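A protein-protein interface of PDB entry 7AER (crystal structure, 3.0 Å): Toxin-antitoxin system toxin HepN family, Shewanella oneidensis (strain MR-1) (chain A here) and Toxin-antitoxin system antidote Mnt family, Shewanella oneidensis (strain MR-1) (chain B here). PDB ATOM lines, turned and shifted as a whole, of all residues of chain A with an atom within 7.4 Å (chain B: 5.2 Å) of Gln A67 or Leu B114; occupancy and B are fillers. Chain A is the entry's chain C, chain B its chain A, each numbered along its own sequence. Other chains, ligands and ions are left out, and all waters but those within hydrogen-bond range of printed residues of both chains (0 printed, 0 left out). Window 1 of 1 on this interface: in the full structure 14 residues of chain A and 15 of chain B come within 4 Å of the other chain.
Of the 13 printed residues of chain B, 8 touch a printed residue of chain A. Hydrophobic or aromatic side chains of chain B that line the printed part of chain A: Val B81, Met B110, His B113 and Leu B114. Of the 14 printed residues of chain A, 10 touch a printed residue of chain B. Printed residues of chain A that touch a printed residue of chain B: Ile A51, Asn A55, Ile A65, Pro A66, Gln A67, Ser A68, Ser A69, Arg A70, Arg A97 and His A102.
Of the printed residues of chain B, Ile A65 touches Arg B118 (3.8 Å). Gln A67 touches just these residues of chain B: Ser B79 (3.6 Å), Thr B80 (3.2 Å), Val B81 (3.1 Å) and Leu B114 (3.5 Å). Asp A71 touches none of the printed residues of chain B. Ser A72 touches none of the printed residues of chain B. Printed residues of chain B within 4 Å of Arg A97: Glu B117 (2.4 Å). Of the printed residues of chain A, Ser B79 touches Gln A67 and Arg A70. Printed residues of chain A within 4 Å of Met B110: His A102. Leu B114 touches one residue of chain A. Of the printed residues of chain A, Arg B118 touches Ile A65 and Pro A66. The nearest residue of chain A that does not touch Leu B114 is Ser A68 (4.1 Å).
O of Gln A67 is in hydrogen-bond range of N of Thr B80, at 3.2 Å. O of Gln A67 lies within hydrogen-bond range of N of Val B81, 3.1 Å away. ND1 of His B113 is in hydrogen-bond range of NE2 of His A102. OE1 of Glu B117 is in hydrogen-bond range of OG of Ser A69, at 2.7 Å. The guanidinium group (NH2) of Arg A97 is in salt-bridge range of the side-chain carboxylate (OE2) of Glu B117 (2.4 Å). O of Pro A66 lies within hydrogen-bond range of NH1 of Arg B118.
The backbone carbonyl oxygen of Ile A51 lies within hydrogen-bond range of the side-chain amide nitrogen of Asn A55, at 3.3 Å. OD1 of Asn A55 is in hydrogen-bond range of OG of Ser A72 (2.6 Å). The backbone NH of Gln A67 lies within hydrogen-bond range of the side-chain carboxylate of Asp A71 (3.1 Å). OG of Ser A68 is in hydrogen-bond range of NH2 of Arg A70, 3.4 Å away. The backbone NH (N) of Asp A71 lies within hydrogen-bond range of the side-chain hydroxyl (OG) of Ser A68, at 3.2 Å. The guanidinium group (NH1) of Arg A97 is in hydrogen-bond range of the side-chain hydroxyl (OG) of Ser A69.
Among the printed residues, merely in contact across the chains: His A102 with Met B110 (3.3 Å), Ser A68 with Thr B80 (3.4 Å), Gln A67 with Leu B114 (3.5 Å), Gln A67 with Ser B79 (3.6 Å), Asn A55 with Glu B117 (3.8 Å), Arg A70 with Ser B79 (3.8 Å), Ile A65 with Arg B118 (3.8 Å) and Ile A51 with Glu B117 (3.9 Å).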
ATOM      1  N   ILE A  51       0.110  16.679  24.816  1.00  0.00           N
ATOM      2  CA  ILE A  51       0.348  17.749  23.850  1.00  0.00           C
ATOM      3  C   ILE A  51       0.046  19.108  24.471  1.00  0.00           C
ATOM      4  O   ILE A  51       0.753  20.093  24.218  1.00  0.00           O
ATOM      5  CB  ILE A  51      -0.482  17.505  22.575  1.00  0.00           C
ATOM      6  CG1 ILE A  51       0.000  16.240  21.862  1.00  0.00           C
ATOM      7  CG2 ILE A  51      -0.398  18.694  21.634  1.00  0.00           C
ATOM      8  CD1 ILE A  51      -0.850  15.848  20.673  1.00  0.00           C
ATOM      9  N   ASN A  55       2.740  22.039  24.760  1.00  0.00           N
ATOM     10  CA  ASN A  55       2.564  23.344  24.130  1.00  0.00           C
ATOM     11  C   ASN A  55       2.524  24.470  25.156  1.00  0.00           C
ATOM     12  O   ASN A  55       2.894  25.606  24.837  1.00  0.00           O
ATOM     13  CB  ASN A  55       1.304  23.366  23.265  1.00  0.00           C
ATOM     14  CG  ASN A  55       1.461  22.553  21.994  1.00  0.00           C
ATOM     15  OD1 ASN A  55       2.535  22.528  21.391  1.00  0.00           O
ATOM     16  ND2 ASN A  55       0.374  21.938  21.545  1.00  0.00           N
ATOM     17  N   GLY A  64       9.682  27.636  20.262  1.00  0.00           N
ATOM     18  CA  GLY A  64       9.494  27.597  18.828  1.00  0.00           C
ATOM     19  C   GLY A  64       8.019  27.508  18.490  1.00  0.00           C
ATOM     20  O   GLY A  64       7.160  27.880  19.284  1.00  0.00           O
ATOM     21  N   ILE A  65       7.743  27.004  17.289  1.00  0.00           N
ATOM     22  CA  ILE A  65       6.385  26.890  16.783  1.00  0.00           C
ATOM     23  C   ILE A  65       6.193  25.496  16.193  1.00  0.00           C
ATOM     24  O   ILE A  65       6.867  25.145  15.217  1.00  0.00           O
ATOM     25  CB  ILE A  65       6.061  27.977  15.748  1.00  0.00           C
ATOM     26  CG1 ILE A  65       5.962  29.334  16.452  1.00  0.00           C
ATOM     27  CG2 ILE A  65       4.771  27.665  15.013  1.00  0.00           C
ATOM     28  CD1 ILE A  65       5.747  30.488  15.538  1.00  0.00           C
ATOM     29  N   PRO A  66       5.310  24.668  16.748  1.00  0.00           N
ATOM     30  CA  PRO A  66       5.181  23.286  16.265  1.00  0.00           C
ATOM     31  C   PRO A  66       4.622  23.247  14.851  1.00  0.00           C
ATOM     32  O   PRO A  66       3.601  23.871  14.553  1.00  0.00           O
ATOM     33  CB  PRO A  66       4.214  22.645  17.270  1.00  0.00           C
ATOM     34  CG  PRO A  66       4.232  23.546  18.469  1.00  0.00           C
ATOM     35  CD  PRO A  66       4.466  24.923  17.929  1.00  0.00           C
ATOM     36  N   GLN A  67       5.309  22.513  13.978  1.00  0.00           N
ATOM     37  CA  GLN A  67       4.826  22.286  12.625  1.00  0.00           C
ATOM     38  C   GLN A  67       3.947  21.049  12.522  1.00  0.00           C
ATOM     39  O   GLN A  67       3.241  20.884  11.521  1.00  0.00           O
ATOM     40  CB  GLN A  67       6.006  22.163  11.658  1.00  0.00           C
ATOM     41  CG  GLN A  67       7.019  23.291  11.774  1.00  0.00           C
ATOM     42  CD  GLN A  67       6.411  24.654  11.509  1.00  0.00           C
ATOM     43  OE1 GLN A  67       6.182  25.031  10.361  1.00  0.00           O
ATOM     44  NE2 GLN A  67       6.144  25.401  12.575  1.00  0.00           N
ATOM     45  N   SER A  68       3.986  20.179  13.528  1.00  0.00           N
ATOM     46  CA  SER A  68       3.083  19.045  13.639  1.00  0.00           C
ATOM     47  C   SER A  68       2.868  18.776  15.123  1.00  0.00           C
ATOM     48  O   SER A  68       3.474  19.422  15.983  1.00  0.00           O
ATOM     49  CB  SER A  68       3.638  17.815  12.913  1.00  0.00           C
ATOM     50  OG  SER A  68       4.773  17.291  13.580  1.00  0.00           O
ATOM     51  N   SER A  69       1.991  17.817  15.427  1.00  0.00           N
ATOM     52  CA  SER A  69       1.791  17.434  16.821  1.00  0.00           C
ATOM     53  C   SER A  69       3.016  16.718  17.375  1.00  0.00           C
ATOM     54  O   SER A  69       3.353  16.873  18.554  1.00  0.00           O
ATOM     55  CB  SER A  69       0.548  16.556  16.959  1.00  0.00           C
ATOM     56  OG  SER A  69      -0.638  17.315  16.804  1.00  0.00           O
ATOM     57  N   ARG A  70       3.692  15.923  16.539  1.00  0.00           N
ATOM     58  CA  ARG A  70       4.952  15.316  16.950  1.00  0.00           C
ATOM     59  C   ARG A  70       5.996  16.378  17.260  1.00  0.00           C
ATOM     60  O   ARG A  70       6.878  16.162  18.099  1.00  0.00           O
ATOM     61  CB  ARG A  70       5.468  14.380  15.855  1.00  0.00           C
ATOM     62  CG  ARG A  70       4.418  13.460  15.256  1.00  0.00           C
ATOM     63  CD  ARG A  70       4.958  12.725  14.036  1.00  0.00           C
ATOM     64  NE  ARG A  70       5.374  13.641  12.975  1.00  0.00           N
ATOM     65  CZ  ARG A  70       4.558  14.133  12.047  1.00  0.00           C
ATOM     66  NH1 ARG A  70       3.274  13.802  12.045  1.00  0.00           N
ATOM     67  NH2 ARG A  70       5.025  14.958  11.120  1.00  0.00           N
ATOM     68  N   ASP A  71       5.899  17.535  16.601  1.00  0.00           N
ATOM     69  CA  ASP A  71       6.901  18.580  16.763  1.00  0.00           C
ATOM     70  C   ASP A  71       6.897  19.155  18.172  1.00  0.00           C
ATOM     71  O   ASP A  71       7.922  19.669  18.635  1.00  0.00           O
ATOM     72  CB  ASP A  71       6.657  19.684  15.734  1.00  0.00           C
ATOM     73  CG  ASP A  71       7.937  20.319  15.251  1.00  0.00           C
ATOM     74  OD1 ASP A  71       8.864  19.567  14.882  1.00  0.00           O
ATOM     75  OD2 ASP A  71       8.014  21.564  15.225  1.00  0.00           O
ATOM     76  N   SER A  72       5.760  19.071  18.867  1.00  0.00           N
ATOM     77  CA  SER A  72       5.663  19.628  20.212  1.00  0.00           C
ATOM     78  C   SER A  72       6.562  18.896  21.200  1.00  0.00           C
ATOM     79  O   SER A  72       7.009  19.495  22.184  1.00  0.00           O
ATOM     80  CB  SER A  72       4.211  19.589  20.689  1.00  0.00           C
ATOM     81  OG  SER A  72       3.415  20.520  19.977  1.00  0.00           O
ATOM     82  N   LEU A  75      10.534  19.702  20.416  1.00  0.00           N
ATOM     83  CA  LEU A  75      10.950  20.988  20.968  1.00  0.00           C
ATOM     84  C   LEU A  75      11.400  20.848  22.416  1.00  0.00           C
ATOM     85  O   LEU A  75      12.373  21.482  22.835  1.00  0.00           O
ATOM     86  CB  LEU A  75       9.812  22.003  20.855  1.00  0.00           C
ATOM     87  CG  LEU A  75       9.517  22.533  19.452  1.00  0.00           C
ATOM     88  CD1 LEU A  75       8.318  23.467  19.471  1.00  0.00           C
ATOM     89  CD2 LEU A  75      10.740  23.239  18.887  1.00  0.00           C
ATOM     90  N   ARG A  97      -2.555   8.160  18.041  1.00  0.00           N
ATOM     91  CA  ARG A  97      -3.674   9.081  18.215  1.00  0.00           C
ATOM     92  C   ARG A  97      -4.207   9.565  16.873  1.00  0.00           C
ATOM     93  O   ARG A  97      -5.423   9.701  16.692  1.00  0.00           O
ATOM     94  CB  ARG A  97      -3.240  10.262  19.083  1.00  0.00           C
ATOM     95  CG  ARG A  97      -4.030  11.541  18.851  1.00  0.00           C
ATOM     96  CD  ARG A  97      -3.413  12.705  19.607  1.00  0.00           C
ATOM     97  NE  ARG A  97      -4.071  13.968  19.302  1.00  0.00           N
ATOM     98  CZ  ARG A  97      -3.612  14.860  18.429  1.00  0.00           C
ATOM     99  NH1 ARG A  97      -2.485  14.627  17.772  1.00  0.00           N
ATOM    100  NH2 ARG A  97      -4.279  15.985  18.218  1.00  0.00           N
ATOM    101  N   HIS A 102      -8.113  10.699  12.905  1.00  0.00           N
ATOM    102  CA  HIS A 102      -8.235  10.807  11.458  1.00  0.00           C
ATOM    103  C   HIS A 102      -8.121   9.423  10.835  1.00  0.00           C
ATOM    104  O   HIS A 102      -7.207   8.660  11.161  1.00  0.00           O
ATOM    105  CB  HIS A 102      -7.165  11.737  10.892  1.00  0.00           C
ATOM    106  CG  HIS A 102      -7.127  13.078  11.554  1.00  0.00           C
ATOM    107  ND1 HIS A 102      -6.132  13.445  12.433  1.00  0.00           N
ATOM    108  CD2 HIS A 102      -7.971  14.134  11.478  1.00  0.00           C
ATOM    109  CE1 HIS A 102      -6.359  14.673  12.864  1.00  0.00           C
ATOM    110  NE2 HIS A 102      -7.470  15.113  12.299  1.00  0.00           N
ATOM    111  N   SER B  79       6.085  17.424   7.958  1.00  0.00           N
ATOM    112  CA  SER B  79       5.265  18.079   8.961  1.00  0.00           C
ATOM    113  C   SER B  79       3.880  18.390   8.404  1.00  0.00           C
ATOM    114  O   SER B  79       3.667  18.453   7.190  1.00  0.00           O
ATOM    115  CB  SER B  79       5.936  19.366   9.447  1.00  0.00           C
ATOM    116  OG  SER B  79       5.794  20.411   8.499  1.00  0.00           O
ATOM    117  N   THR B  80       2.926  18.584   9.318  1.00  0.00           N
ATOM    118  CA  THR B  80       1.557  18.878   8.906  1.00  0.00           C
ATOM    119  C   THR B  80       1.460  20.232   8.211  1.00  0.00           C
ATOM    120  O   THR B  80       0.660  20.393   7.281  1.00  0.00           O
ATOM    121  CB  THR B  80       0.622  18.831  10.116  1.00  0.00           C
ATOM    122  OG1 THR B  80       0.878  17.643  10.876  1.00  0.00           O
ATOM    123  CG2 THR B  80      -0.834  18.830   9.668  1.00  0.00           C
ATOM    124  N   VAL B  81       2.265  21.208   8.637  1.00  0.00           N
ATOM    125  CA  VAL B  81       2.253  22.515   7.989  1.00  0.00           C
ATOM    126  C   VAL B  81       2.757  22.405   6.555  1.00  0.00           C
ATOM    127  O   VAL B  81       2.168  22.978   5.630  1.00  0.00           O
ATOM    128  CB  VAL B  81       3.077  23.525   8.810  1.00  0.00           C
ATOM    129  CG1 VAL B  81       3.210  24.840   8.060  1.00  0.00           C
ATOM    130  CG2 VAL B  81       2.432  23.753  10.168  1.00  0.00           C
ATOM    131  N   MET B 110      -6.246  17.295   9.431  1.00  0.00           N
ATOM    132  CA  MET B 110      -5.171  17.267  10.421  1.00  0.00           C
ATOM    133  C   MET B 110      -4.669  18.675  10.712  1.00  0.00           C
ATOM    134  O   MET B 110      -4.337  19.006  11.852  1.00  0.00           O
ATOM    135  CB  MET B 110      -4.008  16.394   9.949  1.00  0.00           C
ATOM    136  CG  MET B 110      -4.195  14.908  10.194  1.00  0.00           C
ATOM    137  SD  MET B 110      -2.495  13.960  10.299  1.00  0.00           S
ATOM    138  CE  MET B 110      -1.564  14.881   8.849  1.00  0.00           C
ATOM    139  N   TYR B 111      -4.612  19.499   9.664  1.00  0.00           N
ATOM    140  CA  TYR B 111      -4.159  20.875   9.826  1.00  0.00           C
ATOM    141  C   TYR B 111      -5.144  21.685  10.660  1.00  0.00           C
ATOM    142  O   TYR B 111      -4.736  22.537  11.459  1.00  0.00           O
ATOM    143  CB  TYR B 111      -3.950  21.517   8.453  1.00  0.00           C
ATOM    144  CG  TYR B 111      -3.427  22.933   8.499  1.00  0.00           C
ATOM    145  CD1 TYR B 111      -2.075  23.188   8.688  1.00  0.00           C
ATOM    146  CD2 TYR B 111      -4.283  24.016   8.344  1.00  0.00           C
ATOM    147  CE1 TYR B 111      -1.591  24.482   8.729  1.00  0.00           C
ATOM    148  CE2 TYR B 111      -3.808  25.311   8.380  1.00  0.00           C
ATOM    149  CZ  TYR B 111      -2.463  25.540   8.575  1.00  0.00           C
ATOM    150  OH  TYR B 111      -1.987  26.830   8.613  1.00  0.00           O
ATOM    151  N   GLN B 112      -6.443  21.427  10.493  1.00  0.00           N
ATOM    152  CA  GLN B 112      -7.452  22.171  11.244  1.00  0.00           C
ATOM    153  C   GLN B 112      -7.358  21.880  12.737  1.00  0.00           C
ATOM    154  O   GLN B 112      -7.498  22.790  13.563  1.00  0.00           O
ATOM    155  CB  GLN B 112      -8.848  21.840  10.711  1.00  0.00           C
ATOM    156  CG  GLN B 112      -9.147  22.455   9.351  1.00  0.00           C
ATOM    157  CD  GLN B 112     -10.358  21.838   8.673  1.00  0.00           C
ATOM    158  OE1 GLN B 112     -10.863  20.800   9.102  1.00  0.00           O
ATOM    159  NE2 GLN B 112     -10.826  22.476   7.605  1.00  0.00           N
ATOM    160  N   HIS B 113      -7.122  20.618  13.101  1.00  0.00           N
ATOM    161  CA  HIS B 113      -6.918  20.282  14.507  1.00  0.00           C
ATOM    162  C   HIS B 113      -5.642  20.920  15.042  1.00  0.00           C
ATOM    163  O   HIS B 113      -5.636  21.479  16.144  1.00  0.00           O
ATOM    164  CB  HIS B 113      -6.877  18.764  14.687  1.00  0.00           C
ATOM    165  CG  HIS B 113      -8.184  18.086  14.419  1.00  0.00           C
ATOM    166  ND1 HIS B 113      -8.818  18.146  13.196  1.00  0.00           N
ATOM    167  CD2 HIS B 113      -8.975  17.331  15.217  1.00  0.00           C
ATOM    168  CE1 HIS B 113      -9.945  17.458  13.254  1.00  0.00           C
ATOM    169  NE2 HIS B 113     -10.063  16.953  14.469  1.00  0.00           N
ATOM    170  N   LEU B 114      -4.555  20.853  14.268  1.00  0.00           N
ATOM    171  CA  LEU B 114      -3.304  21.482  14.680  1.00  0.00           C
ATOM    172  C   LEU B 114      -3.472  22.985  14.857  1.00  0.00           C
ATOM    173  O   LEU B 114      -2.915  23.572  15.791  1.00  0.00           O
ATOM    174  CB  LEU B 114      -2.207  21.186  13.658  1.00  0.00           C
ATOM    175  CG  LEU B 114      -0.869  21.905  13.860  1.00  0.00           C
ATOM    176  CD1 LEU B 114      -0.195  21.448  15.146  1.00  0.00           C
ATOM    177  CD2 LEU B 114       0.054  21.705  12.664  1.00  0.00           C
ATOM    178  N   GLN B 115      -4.236  23.625  13.967  1.00  0.00           N
ATOM    179  CA  GLN B 115      -4.476  25.059  14.096  1.00  0.00           C
ATOM    180  C   GLN B 115      -5.118  25.391  15.436  1.00  0.00           C
ATOM    181  O   GLN B 115      -4.842  26.445  16.021  1.00  0.00           O
ATOM    182  CB  GLN B 115      -5.352  25.555  12.946  1.00  0.00           C
ATOM    183  CG  GLN B 115      -4.580  25.888  11.684  1.00  0.00           C
ATOM    184  CD  GLN B 115      -3.569  26.998  11.898  1.00  0.00           C
ATOM    185  OE1 GLN B 115      -2.406  26.743  12.213  1.00  0.00           O
ATOM    186  NE2 GLN B 115      -4.009  28.240  11.730  1.00  0.00           N
ATOM    187  N   ALA B 116      -5.972  24.500  15.940  1.00  0.00           N
ATOM    188  CA  ALA B 116      -6.545  24.681  17.268  1.00  0.00           C
ATOM    189  C   ALA B 116      -5.542  24.356  18.366  1.00  0.00           C
ATOM    190  O   ALA B 116      -5.593  24.959  19.443  1.00  0.00           O
ATOM    191  CB  ALA B 116      -7.794  23.816  17.425  1.00  0.00           C
ATOM    192  N   GLU B 117      -4.623  23.420  18.110  1.00  0.00           N
ATOM    193  CA  GLU B 117      -3.657  23.024  19.129  1.00  0.00           C
ATOM    194  C   GLU B 117      -2.664  24.141  19.427  1.00  0.00           C
ATOM    195  O   GLU B 117      -2.340  24.396  20.594  1.00  0.00           O
ATOM    196  CB  GLU B 117      -2.904  21.770  18.686  1.00  0.00           C
ATOM    197  CG  GLU B 117      -3.751  20.517  18.558  1.00  0.00           C
ATOM    198  CD  GLU B 117      -2.928  19.311  18.146  1.00  0.00           C
ATOM    199  OE1 GLU B 117      -1.686  19.434  18.076  1.00  0.00           O
ATOM    200  OE2 GLU B 117      -3.520  18.242  17.891  1.00  0.00           O
ATOM    201  N   ARG B 118      -2.168  24.814  18.390  1.00  0.00           N
ATOM    202  CA  ARG B 118      -1.045  25.736  18.514  1.00  0.00           C
ATOM    203  C   ARG B 118      -1.451  27.201  18.410  1.00  0.00           C
ATOM    204  O   ARG B 118      -0.575  28.063  18.280  1.00  0.00           O
ATOM    205  CB  ARG B 118       0.006  25.422  17.448  1.00  0.00           C
ATOM    206  CG  ARG B 118      -0.517  25.609  16.034  1.00  0.00           C
ATOM    207  CD  ARG B 118       0.586  25.562  14.995  1.00  0.00           C
ATOM    208  NE  ARG B 118       0.080  25.932  13.676  1.00  0.00           N
ATOM    209  CZ  ARG B 118       0.848  26.167  12.617  1.00  0.00           C
ATOM    210  NH1 ARG B 118       2.166  26.078  12.718  1.00  0.00           N
ATOM    211  NH2 ARG B 118       0.296  26.498  11.457  1.00  0.00           N
ATOM    212  N   GLN B 119      -2.749  27.511  18.458  1.00  0.00           N
ATOM    213  CA  GLN B 119      -3.165  28.904  18.329  1.00  0.00           C
ATOM    214  C   GLN B 119      -2.727  29.734  19.528  1.00  0.00           C
ATOM    215  O   GLN B 119      -2.526  30.947  19.401  1.00  0.00           O
ATOM    216  CB  GLN B 119      -4.680  28.992  18.141  1.00  0.00           C
ATOM    217  CG  GLN B 119      -5.163  30.341  17.620  1.00  0.00           C
ATOM    218  CD  GLN B 119      -4.694  30.630  16.203  1.00  0.00           C
ATOM    219  OE1 GLN B 119      -4.266  29.728  15.480  1.00  0.00           O
ATOM    220  NE2 GLN B 119      -4.773  31.892  15.798  1.00  0.00           N
